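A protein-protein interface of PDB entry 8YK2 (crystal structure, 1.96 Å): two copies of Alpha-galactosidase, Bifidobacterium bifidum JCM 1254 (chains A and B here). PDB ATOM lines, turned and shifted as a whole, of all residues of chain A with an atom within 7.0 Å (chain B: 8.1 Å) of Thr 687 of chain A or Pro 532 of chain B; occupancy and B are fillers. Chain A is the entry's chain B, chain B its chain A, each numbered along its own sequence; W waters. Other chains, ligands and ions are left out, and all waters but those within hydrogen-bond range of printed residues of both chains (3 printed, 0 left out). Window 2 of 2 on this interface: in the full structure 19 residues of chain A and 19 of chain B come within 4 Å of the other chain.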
ATOM      1  N   GLN A 609     -31.996  32.982   0.451  1.00  0.00           N
ATOM      2  CA  GLN A 609     -30.823  32.892   1.316  1.00  0.00           C
ATOM      3  C   GLN A 609     -30.350  34.285   1.732  1.00  0.00           C
ATOM      4  O   GLN A 609     -30.198  34.573   2.920  1.00  0.00           O
ATOM      5  CB  GLN A 609     -29.690  32.134   0.613  1.00  0.00           C
ATOM      6  CG  GLN A 609     -28.659  31.514   1.560  1.00  0.00           C
ATOM      7  CD  GLN A 609     -29.024  30.098   1.994  1.00  0.00           C
ATOM      8  OE1 GLN A 609     -29.207  29.822   3.183  1.00  0.00           O
ATOM      9  NE2 GLN A 609     -29.121  29.191   1.027  1.00  0.00           N
ATOM     10  N   VAL A 610     -30.117  35.147   0.742  1.00  0.00           N
ATOM     11  CA  VAL A 610     -29.626  36.502   0.966  1.00  0.00           C
ATOM     12  C   VAL A 610     -30.564  37.484   0.277  1.00  0.00           C
ATOM     13  O   VAL A 610     -30.993  37.255  -0.861  1.00  0.00           O
ATOM     14  CB  VAL A 610     -28.185  36.685   0.444  1.00  0.00           C
ATOM     15  CG1 VAL A 610     -27.506  37.864   1.136  1.00  0.00           C
ATOM     16  CG2 VAL A 610     -27.388  35.406   0.615  1.00  0.00           C
ATOM     17  N   ARG A 614     -28.924  40.740  -7.177  1.00  0.00           N
ATOM     18  CA  ARG A 614     -27.554  40.768  -7.678  1.00  0.00           C
ATOM     19  C   ARG A 614     -27.286  42.152  -8.254  1.00  0.00           C
ATOM     20  O   ARG A 614     -28.182  42.795  -8.807  1.00  0.00           O
ATOM     21  CB  ARG A 614     -27.326  39.684  -8.745  1.00  0.00           C
ATOM     22  CG  ARG A 614     -27.492  38.263  -8.204  1.00  0.00           C
ATOM     23  CD  ARG A 614     -27.520  37.197  -9.310  1.00  0.00           C
ATOM     24  NE  ARG A 614     -27.644  35.856  -8.736  1.00  0.00           N
ATOM     25  CZ  ARG A 614     -27.810  34.749  -9.447  1.00  0.00           C
ATOM     26  NH1 ARG A 614     -27.910  34.786 -10.767  1.00  0.00           N
ATOM     27  NH2 ARG A 614     -27.864  33.576  -8.819  1.00  0.00           N
ATOM     28  N   GLY A 659     -24.061  34.470 -13.460  1.00  0.00           N
ATOM     29  CA  GLY A 659     -25.003  33.403 -13.158  1.00  0.00           C
ATOM     30  C   GLY A 659     -24.993  32.914 -11.727  1.00  0.00           C
ATOM     31  O   GLY A 659     -25.540  31.843 -11.441  1.00  0.00           O
ATOM     32  N   ALA A 660     -24.393  33.676 -10.814  1.00  0.00           N
ATOM     33  CA  ALA A 660     -24.310  33.328  -9.405  1.00  0.00           C
ATOM     34  C   ALA A 660     -24.432  34.611  -8.593  1.00  0.00           C
ATOM     35  O   ALA A 660     -24.263  35.712  -9.120  1.00  0.00           O
ATOM     36  CB  ALA A 660     -22.986  32.604  -9.083  1.00  0.00           C
ATOM     37  N   ASP A 661     -24.714  34.465  -7.291  1.00  0.00           N
ATOM     38  CA  ASP A 661     -24.862  35.641  -6.431  1.00  0.00           C
ATOM     39  C   ASP A 661     -23.567  36.441  -6.337  1.00  0.00           C
ATOM     40  O   ASP A 661     -23.598  37.673  -6.231  1.00  0.00           O
ATOM     41  CB  ASP A 661     -25.314  35.225  -5.029  1.00  0.00           C
ATOM     42  CG  ASP A 661     -26.821  35.065  -4.922  1.00  0.00           C
ATOM     43  OD1 ASP A 661     -27.500  35.031  -5.972  1.00  0.00           O
ATOM     44  OD2 ASP A 661     -27.326  34.987  -3.785  1.00  0.00           O
ATOM     45  N   GLY A 662     -22.421  35.764  -6.346  1.00  0.00           N
ATOM     46  CA  GLY A 662     -21.160  36.472  -6.168  1.00  0.00           C
ATOM     47  C   GLY A 662     -21.061  37.246  -4.865  1.00  0.00           C
ATOM     48  O   GLY A 662     -20.425  38.308  -4.827  1.00  0.00           O
ATOM     49  N   LEU A 663     -21.699  36.755  -3.800  1.00  0.00           N
ATOM     50  CA  LEU A 663     -21.609  37.417  -2.499  1.00  0.00           C
ATOM     51  C   LEU A 663     -20.148  37.578  -2.096  1.00  0.00           C
ATOM     52  O   LEU A 663     -19.377  36.614  -2.131  1.00  0.00           O
ATOM     53  CB  LEU A 663     -22.367  36.603  -1.445  1.00  0.00           C
ATOM     54  CG  LEU A 663     -22.504  37.268  -0.069  1.00  0.00           C
ATOM     55  CD1 LEU A 663     -23.385  38.506  -0.169  1.00  0.00           C
ATOM     56  CD2 LEU A 663     -23.076  36.274   0.942  1.00  0.00           C
ATOM     57  N   SER A 681     -20.897  30.353   5.483  1.00  0.00           N
ATOM     58  CA  SER A 681     -19.821  29.887   4.615  1.00  0.00           C
ATOM     59  C   SER A 681     -20.176  30.177   3.161  1.00  0.00           C
ATOM     60  O   SER A 681     -21.301  29.912   2.733  1.00  0.00           O
ATOM     61  CB  SER A 681     -19.583  28.388   4.818  1.00  0.00           C
ATOM     62  OG  SER A 681     -19.465  28.078   6.203  1.00  0.00           O
ATOM     63  N   VAL A 682     -19.215  30.698   2.405  1.00  0.00           N
ATOM     64  CA  VAL A 682     -19.442  31.196   1.050  1.00  0.00           C
ATOM     65  C   VAL A 682     -18.535  30.423   0.098  1.00  0.00           C
ATOM     66  O   VAL A 682     -17.315  30.405   0.287  1.00  0.00           O
ATOM     67  CB  VAL A 682     -19.171  32.710   0.971  1.00  0.00           C
ATOM     68  CG1 VAL A 682     -19.322  33.223  -0.455  1.00  0.00           C
ATOM     69  CG2 VAL A 682     -20.107  33.467   1.938  1.00  0.00           C
ATOM     70  N   ASP A 683     -19.121  29.792  -0.927  1.00  0.00           N
ATOM     71  CA  ASP A 683     -18.316  29.023  -1.872  1.00  0.00           C
ATOM     72  C   ASP A 683     -17.679  29.957  -2.900  1.00  0.00           C
ATOM     73  O   ASP A 683     -17.797  31.182  -2.825  1.00  0.00           O
ATOM     74  CB  ASP A 683     -19.138  27.898  -2.517  1.00  0.00           C
ATOM     75  CG  ASP A 683     -20.135  28.379  -3.583  1.00  0.00           C
ATOM     76  OD1 ASP A 683     -20.102  29.542  -4.034  1.00  0.00           O
ATOM     77  OD2 ASP A 683     -20.979  27.547  -3.988  1.00  0.00           O
ATOM     78  N   GLN A 684     -17.000  29.375  -3.891  1.00  0.00           N
ATOM     79  CA  GLN A 684     -16.226  30.153  -4.857  1.00  0.00           C
ATOM     80  C   GLN A 684     -17.083  30.945  -5.832  1.00  0.00           C
ATOM     81  O   GLN A 684     -16.568  31.867  -6.473  1.00  0.00           O
ATOM     82  CB  GLN A 684     -15.288  29.239  -5.649  1.00  0.00           C
ATOM     83  CG  GLN A 684     -13.904  29.089  -5.020  1.00  0.00           C
ATOM     84  CD  GLN A 684     -13.935  29.110  -3.500  1.00  0.00           C
ATOM     85  OE1 GLN A 684     -14.590  28.268  -2.864  1.00  0.00           O
ATOM     86  NE2 GLN A 684     -13.238  30.080  -2.905  1.00  0.00           N
ATOM     87  N   ASP A 685     -18.356  30.596  -5.981  1.00  0.00           N
ATOM     88  CA  ASP A 685     -19.278  31.346  -6.822  1.00  0.00           C
ATOM     89  C   ASP A 685     -20.016  32.427  -6.047  1.00  0.00           C
ATOM     90  O   ASP A 685     -20.893  33.092  -6.617  1.00  0.00           O
ATOM     91  CB  ASP A 685     -20.292  30.396  -7.463  1.00  0.00           C
ATOM     92  CG  ASP A 685     -19.623  29.268  -8.232  1.00  0.00           C
ATOM     93  OD1 ASP A 685     -18.649  29.545  -8.954  1.00  0.00           O
ATOM     94  OD2 ASP A 685     -20.059  28.106  -8.099  1.00  0.00           O
ATOM     95  N   GLY A 686     -19.680  32.617  -4.771  1.00  0.00           N
ATOM     96  CA  GLY A 686     -20.392  33.575  -3.952  1.00  0.00           C
ATOM     97  C   GLY A 686     -21.739  33.083  -3.481  1.00  0.00           C
ATOM     98  O   GLY A 686     -22.629  33.898  -3.228  1.00  0.00           O
ATOM     99  N   THR A 687     -21.915  31.765  -3.373  1.00  0.00           N
ATOM    100  CA  THR A 687     -23.137  31.148  -2.877  1.00  0.00           C
ATOM    101  C   THR A 687     -22.909  30.659  -1.449  1.00  0.00           C
ATOM    102  O   THR A 687     -21.867  30.073  -1.150  1.00  0.00           O
ATOM    103  CB  THR A 687     -23.550  29.963  -3.764  1.00  0.00           C
ATOM    104  OG1 THR A 687     -23.648  30.381  -5.136  1.00  0.00           O
ATOM    105  CG2 THR A 687     -24.881  29.399  -3.312  1.00  0.00           C
ATOM    106  N   ILE A 688     -23.891  30.887  -0.580  1.00  0.00           N
ATOM    107  CA  ILE A 688     -23.828  30.438   0.810  1.00  0.00           C
ATOM    108  C   ILE A 688     -24.077  28.935   0.870  1.00  0.00           C
ATOM    109  O   ILE A 688     -25.088  28.445   0.355  1.00  0.00           O
ATOM    110  CB  ILE A 688     -24.855  31.199   1.666  1.00  0.00           C
ATOM    111  CG1 ILE A 688     -24.476  32.681   1.763  1.00  0.00           C
ATOM    112  CG2 ILE A 688     -25.001  30.561   3.055  1.00  0.00           C
ATOM    113  CD1 ILE A 688     -25.371  33.458   2.686  1.00  0.00           C
ATOM    114  N   THR A 689     -23.161  28.194   1.510  1.00  0.00           N
ATOM    115  CA  THR A 689     -23.325  26.751   1.666  1.00  0.00           C
ATOM    116  C   THR A 689     -23.864  26.353   3.033  1.00  0.00           C
ATOM    117  O   THR A 689     -24.430  25.260   3.171  1.00  0.00           O
ATOM    118  CB  THR A 689     -21.988  26.026   1.451  1.00  0.00           C
ATOM    119  OG1 THR A 689     -21.082  26.403   2.489  1.00  0.00           O
ATOM    120  CG2 THR A 689     -21.367  26.383   0.100  1.00  0.00           C
ATOM    121  N   ALA A 690     -23.691  27.195   4.045  1.00  0.00           N
ATOM    122  CA  ALA A 690     -24.081  26.850   5.403  1.00  0.00           C
ATOM    123  C   ALA A 690     -24.096  28.126   6.222  1.00  0.00           C
ATOM    124  O   ALA A 690     -23.365  29.074   5.921  1.00  0.00           O
ATOM    125  CB  ALA A 690     -23.121  25.828   6.029  1.00  0.00           C
ATOM    126  N   THR B 389     -22.208  18.872  -5.832  1.00  0.00           N
ATOM    127  CA  THR B 389     -22.053  20.214  -5.275  1.00  0.00           C
ATOM    128  C   THR B 389     -23.411  20.912  -5.239  1.00  0.00           C
ATOM    129  O   THR B 389     -24.086  21.007  -6.269  1.00  0.00           O
ATOM    130  CB  THR B 389     -21.046  21.031  -6.098  1.00  0.00           C
ATOM    131  OG1 THR B 389     -21.293  20.868  -7.501  1.00  0.00           O
ATOM    132  CG2 THR B 389     -19.634  20.571  -5.807  1.00  0.00           C
ATOM    133  N   LYS B 390     -23.799  21.406  -4.051  1.00  0.00           N
ATOM    134  CA  LYS B 390     -25.141  21.962  -3.842  1.00  0.00           C
ATOM    135  C   LYS B 390     -25.400  23.190  -4.704  1.00  0.00           C
ATOM    136  O   LYS B 390     -26.528  23.400  -5.175  1.00  0.00           O
ATOM    137  CB  LYS B 390     -25.338  22.378  -2.377  1.00  0.00           C
ATOM    138  CG  LYS B 390     -25.253  21.292  -1.339  1.00  0.00           C
ATOM    139  CD  LYS B 390     -25.942  21.754  -0.047  1.00  0.00           C
ATOM    140  CE  LYS B 390     -25.394  23.086   0.455  1.00  0.00           C
ATOM    141  NZ  LYS B 390     -25.828  23.349   1.871  1.00  0.00           N
ATOM    142  N   GLY B 391     -24.392  24.052  -4.845  1.00  0.00           N
ATOM    143  CA  GLY B 391     -24.621  25.369  -5.425  1.00  0.00           C
ATOM    144  C   GLY B 391     -25.106  25.309  -6.861  1.00  0.00           C
ATOM    145  O   GLY B 391     -26.057  25.999  -7.234  1.00  0.00           O
ATOM    146  N   ASP B 392     -24.465  24.481  -7.684  1.00  0.00           N
ATOM    147  CA  ASP B 392     -24.876  24.297  -9.073  1.00  0.00           C
ATOM    148  C   ASP B 392     -25.634  22.991  -9.294  1.00  0.00           C
ATOM    149  O   ASP B 392     -26.130  22.758 -10.404  1.00  0.00           O
ATOM    150  CB  ASP B 392     -23.656  24.374 -10.008  1.00  0.00           C
ATOM    151  CG  ASP B 392     -22.553  23.397  -9.633  1.00  0.00           C
ATOM    152  OD1 ASP B 392     -22.815  22.435  -8.887  1.00  0.00           O
ATOM    153  OD2 ASP B 392     -21.407  23.591 -10.094  1.00  0.00           O
ATOM    154  N   MET B 393     -25.748  22.155  -8.254  1.00  0.00           N
ATOM    155  CA  MET B 393     -26.466  20.875  -8.291  1.00  0.00           C
ATOM    156  C   MET B 393     -25.922  19.958  -9.380  1.00  0.00           C
ATOM    157  O   MET B 393     -26.672  19.231 -10.033  1.00  0.00           O
ATOM    158  CB  MET B 393     -27.977  21.085  -8.448  1.00  0.00           C
ATOM    159  CG  MET B 393     -28.614  21.765  -7.224  1.00  0.00           C
ATOM    160  SD  MET B 393     -28.403  20.798  -5.697  1.00  0.00           S
ATOM    161  CE  MET B 393     -29.360  19.331  -6.060  1.00  0.00           C
ATOM    162  N   SER B 442     -20.689  21.909   1.607  1.00  0.00           N
ATOM    163  CA  SER B 442     -20.822  22.242   0.192  1.00  0.00           C
ATOM    164  C   SER B 442     -21.314  21.067  -0.652  1.00  0.00           C
ATOM    165  O   SER B 442     -21.793  21.275  -1.776  1.00  0.00           O
ATOM    166  CB  SER B 442     -19.478  22.742  -0.343  1.00  0.00           C
ATOM    167  OG  SER B 442     -18.474  21.773  -0.089  1.00  0.00           O
ATOM    168  N   ALA B 498     -31.206  20.691  -3.284  1.00  0.00           N
ATOM    169  CA  ALA B 498     -30.467  20.541  -2.037  1.00  0.00           C
ATOM    170  C   ALA B 498     -30.385  21.886  -1.340  1.00  0.00           C
ATOM    171  O   ALA B 498     -29.354  22.263  -0.772  1.00  0.00           O
ATOM    172  CB  ALA B 498     -29.082  19.940  -2.276  1.00  0.00           C
ATOM    173  N   GLN B 499     -31.488  22.629  -1.403  1.00  0.00           N
ATOM    174  CA  GLN B 499     -31.587  23.977  -0.867  1.00  0.00           C
ATOM    175  C   GLN B 499     -32.578  24.053   0.288  1.00  0.00           C
ATOM    176  O   GLN B 499     -32.220  24.520   1.368  1.00  0.00           O
ATOM    177  CB  GLN B 499     -31.978  24.957  -1.988  1.00  0.00           C
ATOM    178  CG  GLN B 499     -30.809  25.372  -2.893  1.00  0.00           C
ATOM    179  CD  GLN B 499     -30.233  24.218  -3.707  1.00  0.00           C
ATOM    180  OE1 GLN B 499     -30.965  23.459  -4.344  1.00  0.00           O
ATOM    181  NE2 GLN B 499     -28.918  24.082  -3.683  1.00  0.00           N
ATOM    182  N   PRO B 529     -34.795  22.758 -11.037  1.00  0.00           N
ATOM    183  CA  PRO B 529     -33.872  22.436  -9.946  1.00  0.00           C
ATOM    184  C   PRO B 529     -33.546  23.740  -9.228  1.00  0.00           C
ATOM    185  O   PRO B 529     -33.592  24.818  -9.823  1.00  0.00           O
ATOM    186  CB  PRO B 529     -32.649  21.849 -10.665  1.00  0.00           C
ATOM    187  CG  PRO B 529     -32.663  22.567 -12.038  1.00  0.00           C
ATOM    188  CD  PRO B 529     -34.168  22.604 -12.369  1.00  0.00           C
ATOM    189  N   THR B 530     -33.268  23.654  -7.930  1.00  0.00           N
ATOM    190  CA  THR B 530     -33.188  24.875  -7.133  1.00  0.00           C
ATOM    191  C   THR B 530     -31.751  25.348  -6.918  1.00  0.00           C
ATOM    192  O   THR B 530     -31.491  26.116  -5.980  1.00  0.00           O
ATOM    193  CB  THR B 530     -33.918  24.697  -5.796  1.00  0.00           C
ATOM    194  OG1 THR B 530     -33.457  23.520  -5.131  1.00  0.00           O
ATOM    195  CG2 THR B 530     -35.442  24.587  -6.009  1.00  0.00           C
ATOM    196  N   ASN B 531     -30.822  24.930  -7.776  1.00  0.00           N
ATOM    197  CA  ASN B 531     -29.449  25.436  -7.730  1.00  0.00           C
ATOM    198  C   ASN B 531     -29.447  26.960  -7.840  1.00  0.00           C
ATOM    199  O   ASN B 531     -30.004  27.501  -8.808  1.00  0.00           O
ATOM    200  CB  ASN B 531     -28.590  24.841  -8.856  1.00  0.00           C
ATOM    201  CG  ASN B 531     -29.312  24.813 -10.202  1.00  0.00           C
ATOM    202  OD1 ASN B 531     -30.433  24.318 -10.300  1.00  0.00           O
ATOM    203  ND2 ASN B 531     -28.672  25.360 -11.242  1.00  0.00           N
ATOM    204  N   PRO B 532     -28.855  27.682  -6.876  1.00  0.00           N
ATOM    205  CA  PRO B 532     -28.704  29.138  -7.034  1.00  0.00           C
ATOM    206  C   PRO B 532     -27.631  29.516  -8.030  1.00  0.00           C
ATOM    207  O   PRO B 532     -27.667  30.630  -8.563  1.00  0.00           O
ATOM    208  CB  PRO B 532     -28.339  29.616  -5.617  1.00  0.00           C
ATOM    209  CG  PRO B 532     -27.735  28.444  -4.976  1.00  0.00           C
ATOM    210  CD  PRO B 532     -28.388  27.212  -5.559  1.00  0.00           C
ATOM    211  N   THR B 533     -26.683  28.631  -8.306  1.00  0.00           N
ATOM    212  CA  THR B 533     -25.669  28.866  -9.328  1.00  0.00           C
ATOM    213  C   THR B 533     -26.112  28.161 -10.604  1.00  0.00           C
ATOM    214  O   THR B 533     -26.359  26.955 -10.586  1.00  0.00           O
ATOM    215  CB  THR B 533     -24.298  28.340  -8.886  1.00  0.00           C
ATOM    216  OG1 THR B 533     -23.854  29.049  -7.719  1.00  0.00           O
ATOM    217  CG2 THR B 533     -23.271  28.515 -10.007  1.00  0.00           C
ATOM    218  N   VAL B 534     -26.212  28.895 -11.706  1.00  0.00           N
ATOM    219  CA  VAL B 534     -26.607  28.302 -12.980  1.00  0.00           C
ATOM    220  C   VAL B 534     -25.350  28.122 -13.815  1.00  0.00           C
ATOM    221  O   VAL B 534     -24.774  29.098 -14.310  1.00  0.00           O
ATOM    222  CB  VAL B 534     -27.649  29.149 -13.719  1.00  0.00           C
ATOM    223  CG1 VAL B 534     -27.866  28.596 -15.129  1.00  0.00           C
ATOM    224  CG2 VAL B 534     -28.969  29.165 -12.943  1.00  0.00           C
ATOM    225  N   SER B 535     -24.915  26.875 -13.958  1.00  0.00           N
ATOM    226  CA  SER B 535     -23.763  26.588 -14.798  1.00  0.00           C
ATOM    227  C   SER B 535     -24.118  26.833 -16.259  1.00  0.00           C
ATOM    228  O   SER B 535     -25.183  26.417 -16.730  1.00  0.00           O
ATOM    229  CB  SER B 535     -23.304  25.143 -14.604  1.00  0.00           C
ATOM    230  OG  SER B 535     -22.340  24.800 -15.589  1.00  0.00           O
ATOM    231  N   LYS B 562     -35.425  24.798 -16.720  1.00  0.00           N
ATOM    232  CA  LYS B 562     -34.163  25.303 -16.185  1.00  0.00           C
ATOM    233  C   LYS B 562     -33.131  24.179 -16.171  1.00  0.00           C
ATOM    234  O   LYS B 562     -33.381  23.110 -15.601  1.00  0.00           O
ATOM    235  CB  LYS B 562     -34.357  25.862 -14.766  1.00  0.00           C
ATOM    236  CG  LYS B 562     -33.047  26.334 -14.076  1.00  0.00           C
ATOM    237  CD  LYS B 562     -33.274  26.648 -12.600  1.00  0.00           C
ATOM    238  CE  LYS B 562     -31.959  27.020 -11.871  1.00  0.00           C
ATOM    239  NZ  LYS B 562     -32.229  27.131 -10.398  1.00  0.00           N
ATOM    240  N   ASN B 643     -29.978  33.150 -18.794  1.00  0.00           N
ATOM    241  CA  ASN B 643     -28.705  32.453 -18.629  1.00  0.00           C
ATOM    242  C   ASN B 643     -28.334  31.632 -19.855  1.00  0.00           C
ATOM    243  O   ASN B 643     -27.715  30.570 -19.737  1.00  0.00           O
ATOM    244  CB  ASN B 643     -28.734  31.562 -17.385  1.00  0.00           C
ATOM    245  CG  ASN B 643     -28.702  32.368 -16.126  1.00  0.00           C
ATOM    246  OD1 ASN B 643     -27.875  33.256 -15.998  1.00  0.00           O
ATOM    247  ND2 ASN B 643     -29.643  32.121 -15.220  1.00  0.00           N
HETATM  248  O   HOH W   1     -26.307  23.849   5.034  1.00  0.00           O
HETATM  249  O   HOH W   2     -21.814  27.479  -6.506  1.00  0.00           O
HETATM  250  O   HOH W   3     -22.899  26.083  -2.847  1.00  0.00           O
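Thr 687 of chain A touches just these residues of chain B: Pro 532 (3.4 Å) and Thr 533 (2.9 Å).
No residue of chain B comes within 4 Å of Gly 686 of chain A.
Printed residues of chain A within 4 Å of Val 534 of chain B: Gly 659.
Of the printed residues of chain B, Gly 659 of chain A touches Pro 532 (3.8 Å), Thr 533 (3.7 Å) and Val 534 (3.0 Å).
Of the printed residues of chain B, Ala 660 of chain A touches Thr 533 (3.9 Å).
The nearest printed residue of chain B that does not touch Asp 685 of chain A is Asp 392 of chain B (5.1 Å).
The guanidinium group (NE) of Arg 614 of chain A sits at hydrogen-bond distance from the backbone carbonyl oxygen (O) of Ala 660 of chain A, 3.4 Å away.
N of Gly 662 of chain A lies within hydrogen-bond range of O of Asp 685 of chain A (3.1 Å).
The side-chain carboxylate (OD1) of Asp 683 of chain A sits at hydrogen-bond distance from the backbone NH (N) of Asp 685 of chain A, at 2.8 Å.
N of Thr 687 of chain A lies within hydrogen-bond range of OD1 of Asp 683 of chain A.
N of Lys 390 of chain B sits at hydrogen-bond distance from O of Ser 442 of chain B, at 3.0 Å.
ND2 of Asn 531 of chain B is in hydrogen-bond range of O of Thr 533 of chain B, at 2.9 Å.
Of the 17 printed residues of chain B, 4 touch a printed residue of chain A.
Hydrophobic or aromatic side chains of chain A within 4 Å of the printed part of chain B: Ala 660.
Among the printed residues, 9 pairs touch across the chains.
Among the printed residues, no Asp or Glu carboxylate lies within 4 Å of a Lys or Arg side-chain nitrogen of the other chain.
No position is printed for both chains.
Of the 9 pairs that touch across the chains among the printed residues, none has its exchanged pair printed and touching as well.
Among the printed residues, pairs that only touch across the chains: Gly 659 of chain A with Pro 532 of chain B, Gly 659 of chain A with Thr 533 of chain B, Ala 660 of chain A with Thr 533 of chain B, Asp 685 of chain A with Thr 533 of chain B and Thr 687 of chain A with Pro 532 of chain B.
NH2 of Arg 614 of chain A sits at hydrogen-bond distance from O of Pro 532 of chain B (3.0 Å).
The backbone NH (N) of Val 534 of chain B lies within hydrogen-bond range of the backbone carbonyl oxygen (O) of Gly 659 of chain A (3.0 Å).
The side-chain hydroxyl (OG1) of Thr 687 of chain A sits at hydrogen-bond distance from the side-chain hydroxyl (OG1) of Thr 533 of chain B, at 2.9 Å.
The backbone carbonyl oxygen of Thr 689 of chain A sits at hydrogen-bond distance from the side-chain amino group of Lys 390 of chain B, 2.7 Å away.
Water W2 lies within hydrogen-bond range of OD2 of Asp 685 of chain A (2.5 Å), OD2 of Asp 683 of chain A (2.7 Å) and OG1 of Thr 533 of chain B (2.8 Å).
Water W3 lies within hydrogen-bond range of OD2 of Asp 683 of chain A and N of Gly 391 of chain B.
Water W1 lies within hydrogen-bond range of the backbone carbonyl oxygen (O) of Thr 689 of chain A (3.0 Å) and the side-chain amino group (NZ) of Lys 390 of chain B (3.2 Å).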
